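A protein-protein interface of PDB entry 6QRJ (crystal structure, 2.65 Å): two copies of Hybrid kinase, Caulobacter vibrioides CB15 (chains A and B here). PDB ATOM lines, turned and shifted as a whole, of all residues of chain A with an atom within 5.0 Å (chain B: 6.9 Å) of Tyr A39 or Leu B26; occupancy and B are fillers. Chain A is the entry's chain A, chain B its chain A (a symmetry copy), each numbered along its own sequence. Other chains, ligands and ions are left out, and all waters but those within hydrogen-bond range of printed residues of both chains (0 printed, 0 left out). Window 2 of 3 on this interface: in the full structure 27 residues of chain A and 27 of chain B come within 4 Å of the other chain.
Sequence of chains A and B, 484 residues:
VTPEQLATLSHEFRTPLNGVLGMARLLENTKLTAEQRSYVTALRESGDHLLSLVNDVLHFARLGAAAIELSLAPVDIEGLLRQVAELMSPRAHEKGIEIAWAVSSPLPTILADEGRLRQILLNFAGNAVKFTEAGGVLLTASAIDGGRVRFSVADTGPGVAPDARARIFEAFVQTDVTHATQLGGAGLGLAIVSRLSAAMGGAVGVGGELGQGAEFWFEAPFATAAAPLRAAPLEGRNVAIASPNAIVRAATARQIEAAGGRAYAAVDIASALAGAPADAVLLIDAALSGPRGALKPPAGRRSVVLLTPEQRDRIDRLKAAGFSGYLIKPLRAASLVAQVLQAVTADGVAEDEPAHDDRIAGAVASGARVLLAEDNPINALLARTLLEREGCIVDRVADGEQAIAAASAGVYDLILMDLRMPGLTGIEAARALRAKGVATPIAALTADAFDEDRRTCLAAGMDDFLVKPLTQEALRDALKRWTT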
ATOM      1  N   GLU A  35      -4.401   0.228  -3.425  1.00  0.00           N
ATOM      2  CA  GLU A  35      -5.639   1.059  -3.548  1.00  0.00           C
ATOM      3  C   GLU A  35      -6.581   0.382  -4.551  1.00  0.00           C
ATOM      4  O   GLU A  35      -7.622  -0.148  -4.116  1.00  0.00           O
ATOM      5  CB  GLU A  35      -5.330   2.499  -3.984  1.00  0.00           C
ATOM      6  CG  GLU A  35      -4.297   3.202  -3.108  1.00  0.00           C
ATOM      7  CD  GLU A  35      -4.693   3.440  -1.653  1.00  0.00           C
ATOM      8  OE1 GLU A  35      -5.869   3.825  -1.410  1.00  0.00           O
ATOM      9  OE2 GLU A  35      -3.819   3.245  -0.754  1.00  0.00           O
ATOM     10  N   GLN A  36      -6.198   0.341  -5.834  1.00  0.00           N
ATOM     11  CA  GLN A  36      -7.061  -0.167  -6.935  1.00  0.00           C
ATOM     12  C   GLN A  36      -7.338  -1.686  -6.819  1.00  0.00           C
ATOM     13  O   GLN A  36      -8.148  -2.204  -7.616  1.00  0.00           O
ATOM     14  CB  GLN A  36      -6.431   0.194  -8.270  1.00  0.00           C
ATOM     15  CG  GLN A  36      -7.293  -0.213  -9.452  1.00  0.00           C
ATOM     16  CD  GLN A  36      -6.743   0.383 -10.721  1.00  0.00           C
ATOM     17  OE1 GLN A  36      -5.838   1.209 -10.668  1.00  0.00           O
ATOM     18  NE2 GLN A  36      -7.271  -0.038 -11.863  1.00  0.00           N
ATOM     19  N   ARG A  37      -6.678  -2.392  -5.889  1.00  0.00           N
ATOM     20  CA  ARG A  37      -7.080  -3.738  -5.381  1.00  0.00           C
ATOM     21  C   ARG A  37      -7.616  -3.591  -3.951  1.00  0.00           C
ATOM     22  O   ARG A  37      -8.505  -4.391  -3.576  1.00  0.00           O
ATOM     23  CB  ARG A  37      -5.905  -4.722  -5.378  1.00  0.00           C
ATOM     24  CG  ARG A  37      -6.304  -6.151  -5.036  1.00  0.00           C
ATOM     25  CD  ARG A  37      -5.245  -7.155  -5.434  1.00  0.00           C
ATOM     26  NE  ARG A  37      -5.225  -7.383  -6.876  1.00  0.00           N
ATOM     27  CZ  ARG A  37      -6.096  -8.129  -7.558  1.00  0.00           C
ATOM     28  NH1 ARG A  37      -5.971  -8.252  -8.870  1.00  0.00           N
ATOM     29  NH2 ARG A  37      -7.094  -8.736  -6.938  1.00  0.00           N
ATOM     30  N   SER A  38      -7.079  -2.627  -3.187  1.00  0.00           N
ATOM     31  CA  SER A  38      -7.596  -2.203  -1.860  1.00  0.00           C
ATOM     32  C   SER A  38      -9.112  -2.036  -1.944  1.00  0.00           C
ATOM     33  O   SER A  38      -9.803  -2.442  -1.000  1.00  0.00           O
ATOM     34  CB  SER A  38      -6.941  -0.936  -1.368  1.00  0.00           C
ATOM     35  OG  SER A  38      -7.809  -0.231  -0.487  1.00  0.00           O
ATOM     36  N   TYR A  39      -9.588  -1.449  -3.042  1.00  0.00           N
ATOM     37  CA  TYR A  39     -10.991  -1.024  -3.213  1.00  0.00           C
ATOM     38  C   TYR A  39     -11.857  -2.222  -3.558  1.00  0.00           C
ATOM     39  O   TYR A  39     -12.881  -2.295  -2.927  1.00  0.00           O
ATOM     40  CB  TYR A  39     -11.109   0.047  -4.296  1.00  0.00           C
ATOM     41  CG  TYR A  39     -10.395   1.335  -3.982  1.00  0.00           C
ATOM     42  CD1 TYR A  39      -9.888   2.132  -5.007  1.00  0.00           C
ATOM     43  CD2 TYR A  39     -10.211   1.760  -2.665  1.00  0.00           C
ATOM     44  CE1 TYR A  39      -9.204   3.310  -4.734  1.00  0.00           C
ATOM     45  CE2 TYR A  39      -9.554   2.948  -2.378  1.00  0.00           C
ATOM     46  CZ  TYR A  39      -9.056   3.723  -3.418  1.00  0.00           C
ATOM     47  OH  TYR A  39      -8.393   4.886  -3.158  1.00  0.00           O
ATOM     48  N   VAL A  40     -11.436  -3.083  -4.488  1.00  0.00           N
ATOM     49  CA  VAL A  40     -12.238  -4.202  -5.061  1.00  0.00           C
ATOM     50  C   VAL A  40     -12.425  -5.322  -4.037  1.00  0.00           C
ATOM     51  O   VAL A  40     -13.462  -6.031  -4.112  1.00  0.00           O
ATOM     52  CB  VAL A  40     -11.562  -4.765  -6.307  1.00  0.00           C
ATOM     53  CG1 VAL A  40     -12.352  -5.938  -6.856  1.00  0.00           C
ATOM     54  CG2 VAL A  40     -11.386  -3.693  -7.370  1.00  0.00           C
ATOM     55  N   THR A  41     -11.397  -5.542  -3.201  1.00  0.00           N
ATOM     56  CA  THR A  41     -11.455  -6.269  -1.901  1.00  0.00           C
ATOM     57  C   THR A  41     -12.581  -5.620  -1.075  1.00  0.00           C
ATOM     58  O   THR A  41     -13.618  -6.277  -0.976  1.00  0.00           O
ATOM     59  CB  THR A  41     -10.065  -6.333  -1.222  1.00  0.00           C
ATOM     60  OG1 THR A  41      -9.293  -7.323  -1.899  1.00  0.00           O
ATOM     61  CG2 THR A  41     -10.098  -6.665   0.257  1.00  0.00           C
ATOM     62  N   ALA A  42     -12.432  -4.387  -0.569  1.00  0.00           N
ATOM     63  CA  ALA A  42     -13.335  -3.813   0.467  1.00  0.00           C
ATOM     64  C   ALA A  42     -14.762  -3.661  -0.084  1.00  0.00           C
ATOM     65  O   ALA A  42     -15.725  -3.398   0.694  1.00  0.00           O
ATOM     66  CB  ALA A  42     -12.823  -2.498   0.991  1.00  0.00           C
ATOM     67  N   LEU A  43     -14.926  -3.825  -1.387  1.00  0.00           N
ATOM     68  CA  LEU A  43     -16.266  -3.756  -2.004  1.00  0.00           C
ATOM     69  C   LEU A  43     -16.908  -5.135  -1.907  1.00  0.00           C
ATOM     70  O   LEU A  43     -18.110  -5.206  -1.524  1.00  0.00           O
ATOM     71  CB  LEU A  43     -16.117  -3.331  -3.460  1.00  0.00           C
ATOM     72  CG  LEU A  43     -17.427  -3.131  -4.210  1.00  0.00           C
ATOM     73  CD1 LEU A  43     -17.790  -1.662  -4.196  1.00  0.00           C
ATOM     74  CD2 LEU A  43     -17.331  -3.646  -5.640  1.00  0.00           C
ATOM     75  N   LEU B  21     -20.960   1.945  -2.569  1.00  0.00           N
ATOM     76  CA  LEU B  21     -20.953   3.167  -3.412  1.00  0.00           C
ATOM     77  C   LEU B  21     -19.714   4.026  -3.145  1.00  0.00           C
ATOM     78  O   LEU B  21     -19.196   4.606  -4.115  1.00  0.00           O
ATOM     79  CB  LEU B  21     -22.223   3.960  -3.131  1.00  0.00           C
ATOM     80  CG  LEU B  21     -23.526   3.194  -3.357  1.00  0.00           C
ATOM     81  CD1 LEU B  21     -24.700   4.074  -2.953  1.00  0.00           C
ATOM     82  CD2 LEU B  21     -23.655   2.710  -4.800  1.00  0.00           C
ATOM     83  N   GLY B  22     -19.263   4.124  -1.892  1.00  0.00           N
ATOM     84  CA  GLY B  22     -18.007   4.826  -1.563  1.00  0.00           C
ATOM     85  C   GLY B  22     -16.865   4.200  -2.326  1.00  0.00           C
ATOM     86  O   GLY B  22     -16.059   4.893  -2.920  1.00  0.00           O
ATOM     87  N   MET B  23     -16.840   2.888  -2.351  1.00  0.00           N
ATOM     88  CA  MET B  23     -15.781   2.136  -3.046  1.00  0.00           C
ATOM     89  C   MET B  23     -15.902   2.409  -4.541  1.00  0.00           C
ATOM     90  O   MET B  23     -14.885   2.815  -5.115  1.00  0.00           O
ATOM     91  CB  MET B  23     -15.863   0.624  -2.774  1.00  0.00           C
ATOM     92  CG  MET B  23     -15.175   0.157  -1.483  1.00  0.00           C
ATOM     93  SD  MET B  23     -13.694   1.081  -1.032  1.00  0.00           S
ATOM     94  CE  MET B  23     -14.433   2.276   0.092  1.00  0.00           C
ATOM     95  N   ALA B  24     -17.077   2.196  -5.143  1.00  0.00           N
ATOM     96  CA  ALA B  24     -17.332   2.503  -6.576  1.00  0.00           C
ATOM     97  C   ALA B  24     -16.816   3.916  -6.861  1.00  0.00           C
ATOM     98  O   ALA B  24     -16.006   4.063  -7.763  1.00  0.00           O
ATOM     99  CB  ALA B  24     -18.785   2.387  -6.920  1.00  0.00           C
ATOM    100  N   ARG B  25     -17.197   4.904  -6.057  1.00  0.00           N
ATOM    101  CA  ARG B  25     -16.684   6.284  -6.223  1.00  0.00           C
ATOM    102  C   ARG B  25     -15.167   6.204  -6.373  1.00  0.00           C
ATOM    103  O   ARG B  25     -14.690   6.315  -7.494  1.00  0.00           O
ATOM    104  CB  ARG B  25     -17.096   7.192  -5.065  1.00  0.00           C
ATOM    105  CG  ARG B  25     -17.799   8.462  -5.525  1.00  0.00           C
ATOM    106  CD  ARG B  25     -18.591   9.156  -4.426  1.00  0.00           C
ATOM    107  NE  ARG B  25     -20.024   8.900  -4.522  1.00  0.00           N
ATOM    108  CZ  ARG B  25     -20.767   8.234  -3.634  1.00  0.00           C
ATOM    109  NH1 ARG B  25     -22.063   8.080  -3.868  1.00  0.00           N
ATOM    110  NH2 ARG B  25     -20.228   7.729  -2.529  1.00  0.00           N
ATOM    111  N   LEU B  26     -14.438   5.946  -5.292  1.00  0.00           N
ATOM    112  CA  LEU B  26     -12.947   5.970  -5.285  1.00  0.00           C
ATOM    113  C   LEU B  26     -12.398   5.328  -6.549  1.00  0.00           C
ATOM    114  O   LEU B  26     -11.538   5.952  -7.227  1.00  0.00           O
ATOM    115  CB  LEU B  26     -12.443   5.197  -4.079  1.00  0.00           C
ATOM    116  CG  LEU B  26     -12.662   5.901  -2.754  1.00  0.00           C
ATOM    117  CD1 LEU B  26     -12.485   4.915  -1.618  1.00  0.00           C
ATOM    118  CD2 LEU B  26     -11.714   7.076  -2.609  1.00  0.00           C
ATOM    119  N   LEU B  27     -12.856   4.116  -6.837  1.00  0.00           N
ATOM    120  CA  LEU B  27     -12.365   3.363  -8.013  1.00  0.00           C
ATOM    121  C   LEU B  27     -12.359   4.241  -9.273  1.00  0.00           C
ATOM    122  O   LEU B  27     -11.290   4.278  -9.908  1.00  0.00           O
ATOM    123  CB  LEU B  27     -13.193   2.095  -8.207  1.00  0.00           C
ATOM    124  CG  LEU B  27     -12.571   0.870  -7.548  1.00  0.00           C
ATOM    125  CD1 LEU B  27     -13.484  -0.336  -7.635  1.00  0.00           C
ATOM    126  CD2 LEU B  27     -11.224   0.546  -8.176  1.00  0.00           C
ATOM    127  N   GLU B  28     -13.482   4.909  -9.609  1.00  0.00           N
ATOM    128  CA  GLU B  28     -13.686   5.649 -10.896  1.00  0.00           C
ATOM    129  C   GLU B  28     -12.821   6.910 -10.887  1.00  0.00           C
ATOM    130  O   GLU B  28     -12.416   7.297 -11.980  1.00  0.00           O
ATOM    131  CB  GLU B  28     -15.162   5.936 -11.244  1.00  0.00           C
ATOM    132  CG  GLU B  28     -15.807   7.166 -10.590  1.00  0.00           C
ATOM    133  CD  GLU B  28     -17.325   7.275 -10.750  1.00  0.00           C
ATOM    134  OE1 GLU B  28     -17.784   8.345 -11.248  1.00  0.00           O
ATOM    135  OE2 GLU B  28     -18.062   6.303 -10.368  1.00  0.00           O
ATOM    136  N   ASN B  29     -12.475   7.453  -9.712  1.00  0.00           N
ATOM    137  CA  ASN B  29     -11.532   8.599  -9.597  1.00  0.00           C
ATOM    138  C   ASN B  29     -10.081   8.103  -9.502  1.00  0.00           C
ATOM    139  O   ASN B  29      -9.333   8.690  -8.696  1.00  0.00           O
ATOM    140  CB  ASN B  29     -11.908   9.525  -8.436  1.00  0.00           C
ATOM    141  CG  ASN B  29     -11.811  10.988  -8.829  1.00  0.00           C
ATOM    142  OD1 ASN B  29     -10.744  11.608  -8.762  1.00  0.00           O
ATOM    143  ND2 ASN B  29     -12.922  11.547  -9.278  1.00  0.00           N
ATOM    144  N   THR B  30      -9.721   7.075 -10.295  1.00  0.00           N
ATOM    145  CA  THR B  30      -8.359   6.472 -10.478  1.00  0.00           C
ATOM    146  C   THR B  30      -8.274   5.936 -11.928  1.00  0.00           C
ATOM    147  O   THR B  30      -9.297   5.457 -12.461  1.00  0.00           O
ATOM    148  CB  THR B  30      -7.987   5.424  -9.388  1.00  0.00           C
ATOM    149  OG1 THR B  30      -8.656   4.159  -9.504  1.00  0.00           O
ATOM    150  CG2 THR B  30      -8.227   5.895  -7.964  1.00  0.00           C
ATOM    151  N   LEU B  32      -8.129   3.769 -15.118  1.00  0.00           N
ATOM    152  CA  LEU B  32      -8.797   2.443 -15.193  1.00  0.00           C
ATOM    153  C   LEU B  32      -8.559   1.841 -16.576  1.00  0.00           C
ATOM    154  O   LEU B  32      -7.400   1.645 -16.854  1.00  0.00           O
ATOM    155  CB  LEU B  32     -10.282   2.613 -14.862  1.00  0.00           C
ATOM    156  CG  LEU B  32     -10.617   3.072 -13.439  1.00  0.00           C
ATOM    157  CD1 LEU B  32     -12.111   2.958 -13.186  1.00  0.00           C
ATOM    158  CD2 LEU B  32      -9.863   2.266 -12.379  1.00  0.00           C
ATOM    159  N   VAL B  40     -16.783  -0.405 -13.350  1.00  0.00           N
ATOM    160  CA  VAL B  40     -16.988   0.547 -12.221  1.00  0.00           C
ATOM    161  C   VAL B  40     -18.211   1.433 -12.465  1.00  0.00           C
ATOM    162  O   VAL B  40     -18.843   1.864 -11.466  1.00  0.00           O
ATOM    163  CB  VAL B  40     -15.757   1.428 -12.029  1.00  0.00           C
ATOM    164  CG1 VAL B  40     -15.990   2.430 -10.914  1.00  0.00           C
ATOM    165  CG2 VAL B  40     -14.520   0.591 -11.747  1.00  0.00           C
ATOM    166  N   ARG B 454      -8.342  14.785  -0.180  1.00  0.00           N
ATOM    167  CA  ARG B 454      -9.632  14.565  -0.889  1.00  0.00           C
ATOM    168  C   ARG B 454     -10.028  13.084  -1.025  1.00  0.00           C
ATOM    169  O   ARG B 454     -11.178  12.818  -1.437  1.00  0.00           O
ATOM    170  CB  ARG B 454      -9.578  15.237  -2.270  1.00  0.00           C
ATOM    171  CG  ARG B 454      -8.438  14.773  -3.172  1.00  0.00           C
ATOM    172  CD  ARG B 454      -8.372  15.554  -4.479  1.00  0.00           C
ATOM    173  NE  ARG B 454      -8.725  14.757  -5.653  1.00  0.00           N
ATOM    174  CZ  ARG B 454      -9.041  15.251  -6.848  1.00  0.00           C
ATOM    175  NH1 ARG B 454      -9.065  16.557  -7.053  1.00  0.00           N
ATOM    176  NH2 ARG B 454      -9.341  14.425  -7.836  1.00  0.00           N
ATOM    177  N   ARG B 455      -9.153  12.128  -0.725  1.00  0.00           N
ATOM    178  CA  ARG B 455      -9.477  10.690  -0.977  1.00  0.00           C
ATOM    179  C   ARG B 455     -10.541  10.207   0.026  1.00  0.00           C
ATOM    180  O   ARG B 455     -11.336   9.320  -0.368  1.00  0.00           O
ATOM    181  CB  ARG B 455      -8.208   9.834  -0.984  1.00  0.00           C
ATOM    182  CG  ARG B 455      -7.223  10.236  -2.072  1.00  0.00           C
ATOM    183  CD  ARG B 455      -5.934   9.447  -2.036  1.00  0.00           C
ATOM    184  NE  ARG B 455      -4.948  10.046  -2.927  1.00  0.00           N
ATOM    185  CZ  ARG B 455      -3.819   9.462  -3.317  1.00  0.00           C
ATOM    186  NH1 ARG B 455      -3.514   8.242  -2.902  1.00  0.00           N
ATOM    187  NH2 ARG B 455      -2.996  10.107  -4.128  1.00  0.00           N
ATOM    188  N   THR B 456     -10.582  10.779   1.246  1.00  0.00           N
ATOM    189  CA  THR B 456     -11.615  10.505   2.292  1.00  0.00           C
ATOM    190  C   THR B 456     -12.933  11.174   1.904  1.00  0.00           C
ATOM    191  O   THR B 456     -13.992  10.553   2.123  1.00  0.00           O
ATOM    192  CB  THR B 456     -11.274  11.059   3.686  1.00  0.00           C
ATOM    193  OG1 THR B 456      -9.882  11.368   3.757  1.00  0.00           O
ATOM    194  CG2 THR B 456     -11.669  10.109   4.801  1.00  0.00           C
ATOM    195  N   CYS B 457     -12.851  12.415   1.420  1.00  0.00           N
ATOM    196  CA  CYS B 457     -13.985  13.168   0.829  1.00  0.00           C
ATOM    197  C   CYS B 457     -14.869  12.191   0.033  1.00  0.00           C
ATOM    198  O   CYS B 457     -16.077  12.030   0.380  1.00  0.00           O
ATOM    199  CB  CYS B 457     -13.468  14.294  -0.061  1.00  0.00           C
ATOM    200  SG  CYS B 457     -12.380  15.464   0.799  1.00  0.00           S
ATOM    201  N   LEU B 458     -14.274  11.525  -0.961  1.00  0.00           N
ATOM    202  CA  LEU B 458     -14.973  10.606  -1.899  1.00  0.00           C
ATOM    203  C   LEU B 458     -15.714   9.512  -1.114  1.00  0.00           C
ATOM    204  O   LEU B 458     -16.950   9.605  -1.009  1.00  0.00           O
ATOM    205  CB  LEU B 458     -13.937  10.011  -2.860  1.00  0.00           C
ATOM    206  CG  LEU B 458     -13.830  10.660  -4.241  1.00  0.00           C
ATOM    207  CD1 LEU B 458     -12.388  11.050  -4.545  1.00  0.00           C
ATOM    208  CD2 LEU B 458     -14.381   9.726  -5.318  1.00  0.00           C
ATOM    209  N   ALA B 459     -14.963   8.541  -0.564  1.00  0.00           N
ATOM    210  CA  ALA B 459     -15.429   7.388   0.253  1.00  0.00           C
ATOM    211  C   ALA B 459     -16.460   7.806   1.308  1.00  0.00           C
ATOM    212  O   ALA B 459     -17.377   7.001   1.568  1.00  0.00           O
ATOM    213  CB  ALA B 459     -14.250   6.740   0.926  1.00  0.00           C
ATOM    214  N   ALA B 460     -16.273   8.973   1.936  1.00  0.00           N
ATOM    215  CA  ALA B 460     -17.242   9.602   2.861  1.00  0.00           C
ATOM    216  C   ALA B 460     -18.598   9.771   2.169  1.00  0.00           C
ATOM    217  O   ALA B 460     -19.591   9.695   2.898  1.00  0.00           O
ATOM    218  CB  ALA B 460     -16.722  10.925   3.355  1.00  0.00           C
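Of chain B, only Met B23 (3.7 Å), Leu B26 (3.6 Å) and Leu B27 (3.7 Å) come within 4 Å of Tyr A39.
Leu B26 touches just one residue of chain A: Tyr A39 (3.6 Å).
Of the printed residues of chain A, Met B23 touches Tyr A39 and Leu A43.
Printed residues of chain A within 4 Å of Leu B27: Tyr A39 (3.7 Å) and Val A40 (3.97 Å).
Arg B454 touches none of the printed residues of chain A.
The nearest printed residue of chain B that does not touch Leu A43 is Ala B24 (4.04 Å).
Leu B32 touches Gln A36.
Tyr A39 touches Met B23.
Tyr A39 touches Leu B26 (CE2 to CD1, 3.6 Å).
Tyr A39 touches Leu B27.
Leu B27 touches Val A40.
Leu A43 touches Met B23.
OE1 of Glu A35 is in hydrogen-bond range of OH of Tyr A39, 3.2 Å away.
The side-chain hydroxyl (OG1) of Thr B30 sits at hydrogen-bond distance from the backbone carbonyl oxygen (O) of Leu B27.
Position printed for both chains: 40.
Of the 6 pairs that touch across the chains among the printed residues, none has its exchanged pair printed and touching as well.
Hydrophobic or aromatic side chains of chain B that line the printed part of chain A: Met B23, Leu B26, Leu B27 and Leu B32.
Hydrophobic or aromatic side chains of chain A within 4 Å of the printed part of chain B: Tyr A39, Val A40 and Leu A43.
Among the printed residues, 6 pairs touch across the chains.
Among the printed residues, no Asp or Glu carboxylate lies within 4 Å of a Lys or Arg side-chain nitrogen of the other chain.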
